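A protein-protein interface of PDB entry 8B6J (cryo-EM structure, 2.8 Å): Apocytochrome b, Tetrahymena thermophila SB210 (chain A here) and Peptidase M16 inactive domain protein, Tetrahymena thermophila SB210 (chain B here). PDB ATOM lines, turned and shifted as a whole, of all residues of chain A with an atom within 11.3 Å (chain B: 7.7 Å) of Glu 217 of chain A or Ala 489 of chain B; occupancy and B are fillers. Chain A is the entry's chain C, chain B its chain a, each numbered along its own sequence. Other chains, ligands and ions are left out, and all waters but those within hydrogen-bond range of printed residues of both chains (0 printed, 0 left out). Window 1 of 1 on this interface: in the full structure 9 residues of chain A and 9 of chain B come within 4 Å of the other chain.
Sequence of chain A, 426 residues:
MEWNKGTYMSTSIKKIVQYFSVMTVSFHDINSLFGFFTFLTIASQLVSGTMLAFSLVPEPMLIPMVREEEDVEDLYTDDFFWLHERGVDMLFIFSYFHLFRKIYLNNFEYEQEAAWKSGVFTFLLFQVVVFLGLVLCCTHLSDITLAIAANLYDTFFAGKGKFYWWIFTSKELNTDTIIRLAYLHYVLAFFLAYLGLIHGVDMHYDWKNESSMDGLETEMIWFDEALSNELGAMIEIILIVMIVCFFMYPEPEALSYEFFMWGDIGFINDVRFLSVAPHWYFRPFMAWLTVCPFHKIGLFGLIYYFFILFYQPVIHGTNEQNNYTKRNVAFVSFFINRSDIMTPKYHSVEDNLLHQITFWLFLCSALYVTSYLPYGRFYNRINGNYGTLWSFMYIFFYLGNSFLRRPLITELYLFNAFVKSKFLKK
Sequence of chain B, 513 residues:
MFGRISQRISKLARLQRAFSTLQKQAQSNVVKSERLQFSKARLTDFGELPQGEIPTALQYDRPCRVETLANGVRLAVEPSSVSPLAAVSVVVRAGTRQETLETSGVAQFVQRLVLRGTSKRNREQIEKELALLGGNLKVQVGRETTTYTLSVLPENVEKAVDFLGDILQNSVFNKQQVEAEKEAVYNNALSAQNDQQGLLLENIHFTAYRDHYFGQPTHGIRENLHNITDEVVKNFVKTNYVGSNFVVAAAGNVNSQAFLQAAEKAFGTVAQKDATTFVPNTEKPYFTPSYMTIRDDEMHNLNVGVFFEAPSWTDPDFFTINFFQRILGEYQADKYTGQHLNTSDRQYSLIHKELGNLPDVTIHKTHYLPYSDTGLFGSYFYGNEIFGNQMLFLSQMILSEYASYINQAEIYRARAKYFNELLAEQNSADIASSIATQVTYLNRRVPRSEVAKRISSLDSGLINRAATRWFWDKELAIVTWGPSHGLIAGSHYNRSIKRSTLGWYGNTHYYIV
Glu 217 of chain A touches just these residues of chain B: Arg 295 (2.9 Å), Ile 488 (3.5 Å) and Ala 489 (3.7 Å).
Of the printed residues of chain B, Thr 218 of chain A touches Ile 488 (3.4 Å), Ala 489 (3.6 Å) and His 492 (3.8 Å).
Of the printed residues of chain B, Glu 219 of chain A touches Ala 489 (2.9 Å) and His 492 (2.8 Å).
Printed residues of chain B within 4 Å of Glu 225 of chain A: Asn 494 (3.3 Å).
Of the printed residues of chain A, Arg 295 of chain B touches Glu 217 (2.9 Å).
No residue of chain A comes within 4 Å of Gly 486 of chain B.
Leu 487 of chain B touches none of the printed residues of chain A.
Ile 488 of chain B touches two residues of chain A.
Printed residues of chain A within 4 Å of Ala 489 of chain B: Glu 217, Thr 218 and Glu 219.
Ser 491 of chain B touches none of the printed residues of chain A.
His 492 of chain B touches two residues of chain A.
The nearest residue of chain A that does not touch Ala 489 of chain B is Thr 24 of chain A (4.3 Å).
The nearest printed residue of chain A that does not touch Arg 295 of chain B is Thr 218 of chain A (8.1 Å).
The backbone NH of Ile 221 of chain A sits at hydrogen-bond distance from the side-chain carboxylate of Glu 225 of chain A (3.1 Å).
The backbone carbonyl oxygen of His 492 of chain B lies close to the side-chain amide oxygen of Asn 494 of chain B (3.1 Å).
Among the printed residues, pairs that only touch across the chains: Glu 217 of chain A with Ile 488 of chain B, Glu 217 of chain A with Ala 489 of chain B, Thr 218 of chain A with Ile 488 of chain B, Thr 218 of chain A with Ala 489 of chain B, Thr 218 of chain A with His 492 of chain B and Glu 225 of chain A with Asn 494 of chain B.
Hydrophobic or aromatic side chains of chain B that line the printed part of chain A: Ile 488 and His 492.
Among the printed residues, 9 pairs touch across the chains.
O of Ala 489 of chain B lies within hydrogen-bond range of N of Glu 219 of chain A (2.9 Å).
NE2 of His 492 of chain B sits at hydrogen-bond distance from O of Glu 219 of chain A (2.8 Å).
OE1 of Glu 217 of chain A lies within salt-bridge range of NH1 of Arg 295 of chain B.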
ATOM      1  N   SER A  21     -33.121  -0.547  -3.261  1.00  0.00           N
ATOM      2  CA  SER A  21     -32.104  -1.029  -4.185  1.00  0.00           C
ATOM      3  C   SER A  21     -30.922  -1.663  -3.469  1.00  0.00           C
ATOM      4  O   SER A  21     -30.128  -2.357  -4.110  1.00  0.00           O
ATOM      5  CB  SER A  21     -31.610   0.115  -5.072  1.00  0.00           C
ATOM      6  OG  SER A  21     -31.034   1.146  -4.294  1.00  0.00           O
ATOM      7  N   VAL A  22     -30.788  -1.438  -2.162  1.00  0.00           N
ATOM      8  CA  VAL A  22     -29.722  -2.048  -1.376  1.00  0.00           C
ATOM      9  C   VAL A  22     -30.233  -3.115  -0.421  1.00  0.00           C
ATOM     10  O   VAL A  22     -29.415  -3.826   0.183  1.00  0.00           O
ATOM     11  CB  VAL A  22     -28.927  -0.982  -0.593  1.00  0.00           C
ATOM     12  CG1 VAL A  22     -29.732  -0.485   0.597  1.00  0.00           C
ATOM     13  CG2 VAL A  22     -27.590  -1.532  -0.146  1.00  0.00           C
ATOM     14  N   MET A  23     -31.548  -3.256  -0.268  1.00  0.00           N
ATOM     15  CA  MET A  23     -32.100  -4.216   0.679  1.00  0.00           C
ATOM     16  C   MET A  23     -31.711  -5.637   0.294  1.00  0.00           C
ATOM     17  O   MET A  23     -31.659  -5.987  -0.887  1.00  0.00           O
ATOM     18  CB  MET A  23     -33.623  -4.088   0.718  1.00  0.00           C
ATOM     19  CG  MET A  23     -34.302  -4.908   1.798  1.00  0.00           C
ATOM     20  SD  MET A  23     -35.915  -5.508   1.270  1.00  0.00           S
ATOM     21  CE  MET A  23     -36.630  -4.014   0.592  1.00  0.00           C
ATOM     22  N   THR A  24     -31.443  -6.459   1.304  1.00  0.00           N
ATOM     23  CA  THR A  24     -31.136  -7.868   1.118  1.00  0.00           C
ATOM     24  C   THR A  24     -32.142  -8.715   1.885  1.00  0.00           C
ATOM     25  O   THR A  24     -32.624  -8.320   2.952  1.00  0.00           O
ATOM     26  CB  THR A  24     -29.718  -8.204   1.588  1.00  0.00           C
ATOM     27  OG1 THR A  24     -29.588  -7.902   2.983  1.00  0.00           O
ATOM     28  CG2 THR A  24     -28.689  -7.409   0.799  1.00  0.00           C
ATOM     29  N   VAL A  25     -32.456  -9.882   1.334  1.00  0.00           N
ATOM     30  CA  VAL A  25     -33.441 -10.793   1.902  1.00  0.00           C
ATOM     31  C   VAL A  25     -32.769 -12.136   2.148  1.00  0.00           C
ATOM     32  O   VAL A  25     -32.149 -12.701   1.240  1.00  0.00           O
ATOM     33  CB  VAL A  25     -34.659 -10.958   0.976  1.00  0.00           C
ATOM     34  CG1 VAL A  25     -35.708 -11.840   1.632  1.00  0.00           C
ATOM     35  CG2 VAL A  25     -35.242  -9.602   0.618  1.00  0.00           C
ATOM     36  N   SER A  26     -32.893 -12.642   3.371  1.00  0.00           N
ATOM     37  CA  SER A  26     -32.370 -13.962   3.686  1.00  0.00           C
ATOM     38  C   SER A  26     -33.193 -15.037   2.986  1.00  0.00           C
ATOM     39  O   SER A  26     -34.370 -14.845   2.671  1.00  0.00           O
ATOM     40  CB  SER A  26     -32.379 -14.195   5.197  1.00  0.00           C
ATOM     41  OG  SER A  26     -33.682 -14.031   5.728  1.00  0.00           O
ATOM     42  N   PHE A  27     -32.556 -16.178   2.733  1.00  0.00           N
ATOM     43  CA  PHE A  27     -33.229 -17.264   2.035  1.00  0.00           C
ATOM     44  C   PHE A  27     -34.471 -17.697   2.804  1.00  0.00           C
ATOM     45  O   PHE A  27     -34.444 -17.845   4.028  1.00  0.00           O
ATOM     46  CB  PHE A  27     -32.272 -18.439   1.849  1.00  0.00           C
ATOM     47  CG  PHE A  27     -31.066 -18.102   1.020  1.00  0.00           C
ATOM     48  CD1 PHE A  27     -31.123 -18.156  -0.360  1.00  0.00           C
ATOM     49  CD2 PHE A  27     -29.881 -17.719   1.622  1.00  0.00           C
ATOM     50  CE1 PHE A  27     -30.020 -17.841  -1.123  1.00  0.00           C
ATOM     51  CE2 PHE A  27     -28.775 -17.404   0.862  1.00  0.00           C
ATOM     52  CZ  PHE A  27     -28.845 -17.464  -0.511  1.00  0.00           C
ATOM     53  N   HIS A 204     -38.667  -5.094   8.499  1.00  0.00           N
ATOM     54  CA  HIS A 204     -37.388  -5.651   8.072  1.00  0.00           C
ATOM     55  C   HIS A 204     -36.383  -5.733   9.212  1.00  0.00           C
ATOM     56  O   HIS A 204     -35.371  -6.430   9.082  1.00  0.00           O
ATOM     57  CB  HIS A 204     -36.809  -4.813   6.933  1.00  0.00           C
ATOM     58  CG  HIS A 204     -35.480  -5.295   6.443  1.00  0.00           C
ATOM     59  ND1 HIS A 204     -34.287  -4.774   6.896  1.00  0.00           N
ATOM     60  CD2 HIS A 204     -35.154  -6.251   5.541  1.00  0.00           C
ATOM     61  CE1 HIS A 204     -33.284  -5.387   6.293  1.00  0.00           C
ATOM     62  NE2 HIS A 204     -33.784  -6.288   5.466  1.00  0.00           N
ATOM     63  N   TRP A 207     -36.841  -9.516  10.484  1.00  0.00           N
ATOM     64  CA  TRP A 207     -37.534 -10.451   9.611  1.00  0.00           C
ATOM     65  C   TRP A 207     -36.756 -11.758   9.523  1.00  0.00           C
ATOM     66  O   TRP A 207     -35.550 -11.757   9.259  1.00  0.00           O
ATOM     67  CB  TRP A 207     -37.711  -9.849   8.220  1.00  0.00           C
ATOM     68  CG  TRP A 207     -38.530 -10.699   7.311  1.00  0.00           C
ATOM     69  CD1 TRP A 207     -39.886 -10.711   7.207  1.00  0.00           C
ATOM     70  CD2 TRP A 207     -38.048 -11.667   6.373  1.00  0.00           C
ATOM     71  NE1 TRP A 207     -40.283 -11.624   6.263  1.00  0.00           N
ATOM     72  CE2 TRP A 207     -39.171 -12.225   5.736  1.00  0.00           C
ATOM     73  CE3 TRP A 207     -36.775 -12.115   6.010  1.00  0.00           C
ATOM     74  CZ2 TRP A 207     -39.061 -13.206   4.757  1.00  0.00           C
ATOM     75  CZ3 TRP A 207     -36.669 -13.089   5.039  1.00  0.00           C
ATOM     76  CH2 TRP A 207     -37.804 -13.624   4.424  1.00  0.00           C
ATOM     77  N   MET A 213     -32.907 -19.958  14.420  1.00  0.00           N
ATOM     78  CA  MET A 213     -31.967 -18.967  13.903  1.00  0.00           C
ATOM     79  C   MET A 213     -30.886 -19.683  13.106  1.00  0.00           C
ATOM     80  O   MET A 213     -29.941 -20.234  13.673  1.00  0.00           O
ATOM     81  CB  MET A 213     -31.369 -18.157  15.048  1.00  0.00           C
ATOM     82  CG  MET A 213     -30.338 -17.125  14.620  1.00  0.00           C
ATOM     83  SD  MET A 213     -28.651 -17.759  14.606  1.00  0.00           S
ATOM     84  CE  MET A 213     -27.751 -16.304  14.083  1.00  0.00           C
ATOM     85  N   ASP A 214     -31.023 -19.680  11.783  1.00  0.00           N
ATOM     86  CA  ASP A 214     -29.957 -20.179  10.928  1.00  0.00           C
ATOM     87  C   ASP A 214     -28.778 -19.216  10.954  1.00  0.00           C
ATOM     88  O   ASP A 214     -28.953 -17.995  10.921  1.00  0.00           O
ATOM     89  CB  ASP A 214     -30.460 -20.356   9.497  1.00  0.00           C
ATOM     90  CG  ASP A 214     -30.931 -19.055   8.882  1.00  0.00           C
ATOM     91  OD1 ASP A 214     -31.318 -18.145   9.643  1.00  0.00           O
ATOM     92  OD2 ASP A 214     -30.920 -18.943   7.639  1.00  0.00           O
ATOM     93  N   GLY A 215     -27.571 -19.767  11.008  1.00  0.00           N
ATOM     94  CA  GLY A 215     -26.381 -18.947  11.113  1.00  0.00           C
ATOM     95  C   GLY A 215     -25.879 -18.441   9.777  1.00  0.00           C
ATOM     96  O   GLY A 215     -24.674 -18.245   9.596  1.00  0.00           O
ATOM     97  N   LEU A 216     -26.790 -18.221   8.834  1.00  0.00           N
ATOM     98  CA  LEU A 216     -26.429 -17.764   7.501  1.00  0.00           C
ATOM     99  C   LEU A 216     -26.301 -16.247   7.492  1.00  0.00           C
ATOM    100  O   LEU A 216     -27.207 -15.537   7.938  1.00  0.00           O
ATOM    101  CB  LEU A 216     -27.470 -18.210   6.475  1.00  0.00           C
ATOM    102  CG  LEU A 216     -27.727 -19.716   6.397  1.00  0.00           C
ATOM    103  CD1 LEU A 216     -28.690 -20.026   5.263  1.00  0.00           C
ATOM    104  CD2 LEU A 216     -26.427 -20.484   6.224  1.00  0.00           C
ATOM    105  N   GLU A 217     -25.173 -15.758   6.980  1.00  0.00           N
ATOM    106  CA  GLU A 217     -24.923 -14.327   6.873  1.00  0.00           C
ATOM    107  C   GLU A 217     -25.155 -13.786   5.472  1.00  0.00           C
ATOM    108  O   GLU A 217     -25.591 -12.640   5.329  1.00  0.00           O
ATOM    109  CB  GLU A 217     -23.486 -14.013   7.298  1.00  0.00           C
ATOM    110  CG  GLU A 217     -23.201 -14.311   8.759  1.00  0.00           C
ATOM    111  CD  GLU A 217     -21.750 -14.092   9.125  1.00  0.00           C
ATOM    112  OE1 GLU A 217     -20.937 -13.844   8.210  1.00  0.00           O
ATOM    113  OE2 GLU A 217     -21.421 -14.164  10.327  1.00  0.00           O
ATOM    114  N   THR A 218     -24.879 -14.579   4.441  1.00  0.00           N
ATOM    115  CA  THR A 218     -25.154 -14.157   3.078  1.00  0.00           C
ATOM    116  C   THR A 218     -26.657 -14.045   2.853  1.00  0.00           C
ATOM    117  O   THR A 218     -27.457 -14.741   3.482  1.00  0.00           O
ATOM    118  CB  THR A 218     -24.552 -15.140   2.077  1.00  0.00           C
ATOM    119  OG1 THR A 218     -25.039 -16.460   2.349  1.00  0.00           O
ATOM    120  CG2 THR A 218     -23.036 -15.131   2.167  1.00  0.00           C
ATOM    121  N   GLU A 219     -27.037 -13.152   1.943  1.00  0.00           N
ATOM    122  CA  GLU A 219     -28.442 -12.888   1.675  1.00  0.00           C
ATOM    123  C   GLU A 219     -28.616 -12.557   0.202  1.00  0.00           C
ATOM    124  O   GLU A 219     -27.664 -12.198  -0.493  1.00  0.00           O
ATOM    125  CB  GLU A 219     -28.971 -11.737   2.540  1.00  0.00           C
ATOM    126  CG  GLU A 219     -28.849 -11.972   4.035  1.00  0.00           C
ATOM    127  CD  GLU A 219     -29.311 -10.780   4.848  1.00  0.00           C
ATOM    128  OE1 GLU A 219     -29.532  -9.705   4.255  1.00  0.00           O
ATOM    129  OE2 GLU A 219     -29.452 -10.920   6.081  1.00  0.00           O
ATOM    130  N   MET A 220     -29.852 -12.690  -0.265  1.00  0.00           N
ATOM    131  CA  MET A 220     -30.197 -12.333  -1.631  1.00  0.00           C
ATOM    132  C   MET A 220     -30.354 -10.822  -1.759  1.00  0.00           C
ATOM    133  O   MET A 220     -30.490 -10.099  -0.769  1.00  0.00           O
ATOM    134  CB  MET A 220     -31.495 -13.019  -2.050  1.00  0.00           C
ATOM    135  CG  MET A 220     -31.466 -14.531  -1.953  1.00  0.00           C
ATOM    136  SD  MET A 220     -33.051 -15.213  -1.429  1.00  0.00           S
ATOM    137  CE  MET A 220     -34.166 -14.365  -2.540  1.00  0.00           C
ATOM    138  N   ILE A 221     -30.327 -10.346  -2.998  1.00  0.00           N
ATOM    139  CA  ILE A 221     -30.660  -8.959  -3.300  1.00  0.00           C
ATOM    140  C   ILE A 221     -32.138  -8.902  -3.652  1.00  0.00           C
ATOM    141  O   ILE A 221     -32.623  -9.698  -4.465  1.00  0.00           O
ATOM    142  CB  ILE A 221     -29.788  -8.415  -4.444  1.00  0.00           C
ATOM    143  CG1 ILE A 221     -29.902  -6.890  -4.529  1.00  0.00           C
ATOM    144  CG2 ILE A 221     -30.191  -9.033  -5.770  1.00  0.00           C
ATOM    145  CD1 ILE A 221     -29.277  -6.161  -3.359  1.00  0.00           C
ATOM    146  N   TRP A 222     -32.864  -7.973  -3.030  1.00  0.00           N
ATOM    147  CA  TRP A 222     -34.319  -8.003  -3.130  1.00  0.00           C
ATOM    148  C   TRP A 222     -34.801  -7.759  -4.553  1.00  0.00           C
ATOM    149  O   TRP A 222     -35.759  -8.398  -5.002  1.00  0.00           O
ATOM    150  CB  TRP A 222     -34.944  -6.973  -2.192  1.00  0.00           C
ATOM    151  CG  TRP A 222     -36.432  -6.902  -2.350  1.00  0.00           C
ATOM    152  CD1 TRP A 222     -37.355  -7.711  -1.760  1.00  0.00           C
ATOM    153  CD2 TRP A 222     -37.168  -5.981  -3.165  1.00  0.00           C
ATOM    154  NE1 TRP A 222     -38.620  -7.351  -2.153  1.00  0.00           N
ATOM    155  CE2 TRP A 222     -38.532  -6.290  -3.015  1.00  0.00           C
ATOM    156  CE3 TRP A 222     -36.805  -4.925  -4.005  1.00  0.00           C
ATOM    157  CZ2 TRP A 222     -39.534  -5.582  -3.672  1.00  0.00           C
ATOM    158  CZ3 TRP A 222     -37.801  -4.223  -4.656  1.00  0.00           C
ATOM    159  CH2 TRP A 222     -39.149  -4.554  -4.487  1.00  0.00           C
ATOM    160  N   GLU A 225     -33.630 -11.105  -7.228  1.00  0.00           N
ATOM    161  CA  GLU A 225     -33.551 -12.457  -6.684  1.00  0.00           C
ATOM    162  C   GLU A 225     -34.757 -12.768  -5.808  1.00  0.00           C
ATOM    163  O   GLU A 225     -35.391 -13.818  -5.960  1.00  0.00           O
ATOM    164  CB  GLU A 225     -32.251 -12.628  -5.902  1.00  0.00           C
ATOM    165  CG  GLU A 225     -31.008 -12.457  -6.754  1.00  0.00           C
ATOM    166  CD  GLU A 225     -29.730 -12.583  -5.954  1.00  0.00           C
ATOM    167  OE1 GLU A 225     -29.807 -12.865  -4.741  1.00  0.00           O
ATOM    168  OE2 GLU A 225     -28.646 -12.395  -6.542  1.00  0.00           O
ATOM    169  N   TYR B 291     -15.150 -15.626  -5.737  1.00  0.00           N
ATOM    170  CA  TYR B 291     -15.195 -14.498  -4.811  1.00  0.00           C
ATOM    171  C   TYR B 291     -14.782 -15.017  -3.441  1.00  0.00           C
ATOM    172  O   TYR B 291     -15.563 -15.703  -2.775  1.00  0.00           O
ATOM    173  CB  TYR B 291     -16.592 -13.873  -4.775  1.00  0.00           C
ATOM    174  CG  TYR B 291     -16.762 -12.670  -3.859  1.00  0.00           C
ATOM    175  CD1 TYR B 291     -15.705 -12.167  -3.109  1.00  0.00           C
ATOM    176  CD2 TYR B 291     -17.994 -12.044  -3.743  1.00  0.00           C
ATOM    177  CE1 TYR B 291     -15.873 -11.081  -2.277  1.00  0.00           C
ATOM    178  CE2 TYR B 291     -18.169 -10.955  -2.915  1.00  0.00           C
ATOM    179  CZ  TYR B 291     -17.107 -10.479  -2.184  1.00  0.00           C
ATOM    180  OH  TYR B 291     -17.278  -9.394  -1.356  1.00  0.00           O
ATOM    181  N   ARG B 295     -12.125 -12.884   6.021  1.00  0.00           N
ATOM    182  CA  ARG B 295     -12.728 -11.989   6.999  1.00  0.00           C
ATOM    183  C   ARG B 295     -11.830 -11.876   8.223  1.00  0.00           C
ATOM    184  O   ARG B 295     -11.581 -12.870   8.914  1.00  0.00           O
ATOM    185  CB  ARG B 295     -14.113 -12.491   7.399  1.00  0.00           C
ATOM    186  CG  ARG B 295     -14.829 -11.570   8.367  1.00  0.00           C
ATOM    187  CD  ARG B 295     -16.266 -11.990   8.593  1.00  0.00           C
ATOM    188  NE  ARG B 295     -16.983 -11.020   9.411  1.00  0.00           N
ATOM    189  CZ  ARG B 295     -18.239 -11.156   9.809  1.00  0.00           C
ATOM    190  NH1 ARG B 295     -18.954 -12.222   9.492  1.00  0.00           N
ATOM    191  NH2 ARG B 295     -18.794 -10.197  10.544  1.00  0.00           N
ATOM    192  N   SER B 484     -15.099  -7.627   7.088  1.00  0.00           N
ATOM    193  CA  SER B 484     -16.112  -7.903   6.080  1.00  0.00           C
ATOM    194  C   SER B 484     -17.523  -7.860   6.652  1.00  0.00           C
ATOM    195  O   SER B 484     -18.440  -8.443   6.068  1.00  0.00           O
ATOM    196  CB  SER B 484     -15.849  -9.260   5.427  1.00  0.00           C
ATOM    197  OG  SER B 484     -14.564  -9.299   4.832  1.00  0.00           O
ATOM    198  N   HIS B 485     -17.720  -7.169   7.776  1.00  0.00           N
ATOM    199  CA  HIS B 485     -19.047  -7.106   8.377  1.00  0.00           C
ATOM    200  C   HIS B 485     -20.062  -6.518   7.406  1.00  0.00           C
ATOM    201  O   HIS B 485     -21.200  -6.993   7.320  1.00  0.00           O
ATOM    202  CB  HIS B 485     -18.996  -6.287   9.665  1.00  0.00           C
ATOM    203  CG  HIS B 485     -20.341  -6.003  10.254  1.00  0.00           C
ATOM    204  ND1 HIS B 485     -21.386  -6.900  10.195  1.00  0.00           N
ATOM    205  CD2 HIS B 485     -20.812  -4.922  10.920  1.00  0.00           C
ATOM    206  CE1 HIS B 485     -22.443  -6.383  10.794  1.00  0.00           C
ATOM    207  NE2 HIS B 485     -22.121  -5.183  11.244  1.00  0.00           N
ATOM    208  N   GLY B 486     -19.673  -5.474   6.674  1.00  0.00           N
ATOM    209  CA  GLY B 486     -20.573  -4.900   5.688  1.00  0.00           C
ATOM    210  C   GLY B 486     -20.809  -5.812   4.499  1.00  0.00           C
ATOM    211  O   GLY B 486     -21.915  -5.859   3.953  1.00  0.00           O
ATOM    212  N   LEU B 487     -19.780  -6.544   4.079  1.00  0.00           N
ATOM    213  CA  LEU B 487     -19.805  -7.274   2.817  1.00  0.00           C
ATOM    214  C   LEU B 487     -20.283  -8.717   2.946  1.00  0.00           C
ATOM    215  O   LEU B 487     -20.418  -9.394   1.923  1.00  0.00           O
ATOM    216  CB  LEU B 487     -18.408  -7.262   2.187  1.00  0.00           C
ATOM    217  CG  LEU B 487     -17.853  -5.885   1.816  1.00  0.00           C
ATOM    218  CD1 LEU B 487     -16.397  -5.990   1.404  1.00  0.00           C
ATOM    219  CD2 LEU B 487     -18.676  -5.257   0.704  1.00  0.00           C
ATOM    220  N   ILE B 488     -20.548  -9.208   4.158  1.00  0.00           N
ATOM    221  CA  ILE B 488     -20.972 -10.599   4.304  1.00  0.00           C
ATOM    222  C   ILE B 488     -22.278 -10.840   3.557  1.00  0.00           C
ATOM    223  O   ILE B 488     -22.486 -11.908   2.972  1.00  0.00           O
ATOM    224  CB  ILE B 488     -21.100 -10.982   5.791  1.00  0.00           C
ATOM    225  CG1 ILE B 488     -22.054 -10.028   6.517  1.00  0.00           C
ATOM    226  CG2 ILE B 488     -19.733 -11.009   6.453  1.00  0.00           C
ATOM    227  CD1 ILE B 488     -22.210 -10.323   7.993  1.00  0.00           C
ATOM    228  N   ALA B 489     -23.176  -9.853   3.565  1.00  0.00           N
ATOM    229  CA  ALA B 489     -24.484 -10.044   2.947  1.00  0.00           C
ATOM    230  C   ALA B 489     -24.357 -10.373   1.465  1.00  0.00           C
ATOM    231  O   ALA B 489     -25.079 -11.232   0.948  1.00  0.00           O
ATOM    232  CB  ALA B 489     -25.341  -8.795   3.144  1.00  0.00           C
ATOM    233  N   GLY B 490     -23.451  -9.696   0.764  1.00  0.00           N
ATOM    234  CA  GLY B 490     -23.252  -9.929  -0.652  1.00  0.00           C
ATOM    235  C   GLY B 490     -21.972 -10.680  -0.953  1.00  0.00           C
ATOM    236  O   GLY B 490     -21.425 -10.571  -2.053  1.00  0.00           O
ATOM    237  N   SER B 491     -21.486 -11.449   0.021  1.00  0.00           N
ATOM    238  CA  SER B 491     -20.209 -12.137  -0.122  1.00  0.00           C
ATOM    239  C   SER B 491     -20.237 -13.240  -1.170  1.00  0.00           C
ATOM    240  O   SER B 491     -19.170 -13.757  -1.519  1.00  0.00           O
ATOM    241  CB  SER B 491     -19.782 -12.724   1.224  1.00  0.00           C
ATOM    242  OG  SER B 491     -18.527 -13.372   1.118  1.00  0.00           O
ATOM    243  N   HIS B 492     -21.408 -13.622  -1.668  1.00  0.00           N
ATOM    244  CA  HIS B 492     -21.518 -14.674  -2.667  1.00  0.00           C
ATOM    245  C   HIS B 492     -21.611 -14.077  -4.066  1.00  0.00           C
ATOM    246  O   HIS B 492     -22.040 -12.936  -4.250  1.00  0.00           O
ATOM    247  CB  HIS B 492     -22.732 -15.567  -2.393  1.00  0.00           C
ATOM    248  CG  HIS B 492     -24.023 -14.822  -2.238  1.00  0.00           C
ATOM    249  ND1 HIS B 492     -24.202 -13.527  -2.675  1.00  0.00           N
ATOM    250  CD2 HIS B 492     -25.203 -15.198  -1.689  1.00  0.00           C
ATOM    251  CE1 HIS B 492     -25.434 -13.138  -2.404  1.00  0.00           C
ATOM    252  NE2 HIS B 492     -26.063 -14.133  -1.806  1.00  0.00           N
ATOM    253  N   ASN B 494     -23.295 -13.228  -6.917  1.00  0.00           N
ATOM    254  CA  ASN B 494     -24.728 -13.089  -7.152  1.00  0.00           C
ATOM    255  C   ASN B 494     -25.017 -12.081  -8.257  1.00  0.00           C
ATOM    256  O   ASN B 494     -24.104 -11.640  -8.961  1.00  0.00           O
ATOM    257  CB  ASN B 494     -25.433 -12.677  -5.857  1.00  0.00           C
ATOM    258  CG  ASN B 494     -24.971 -11.331  -5.341  1.00  0.00           C
ATOM    259  OD1 ASN B 494     -23.856 -10.895  -5.623  1.00  0.00           O
ATOM    260  ND2 ASN B 494     -25.826 -10.667  -4.573  1.00  0.00           N
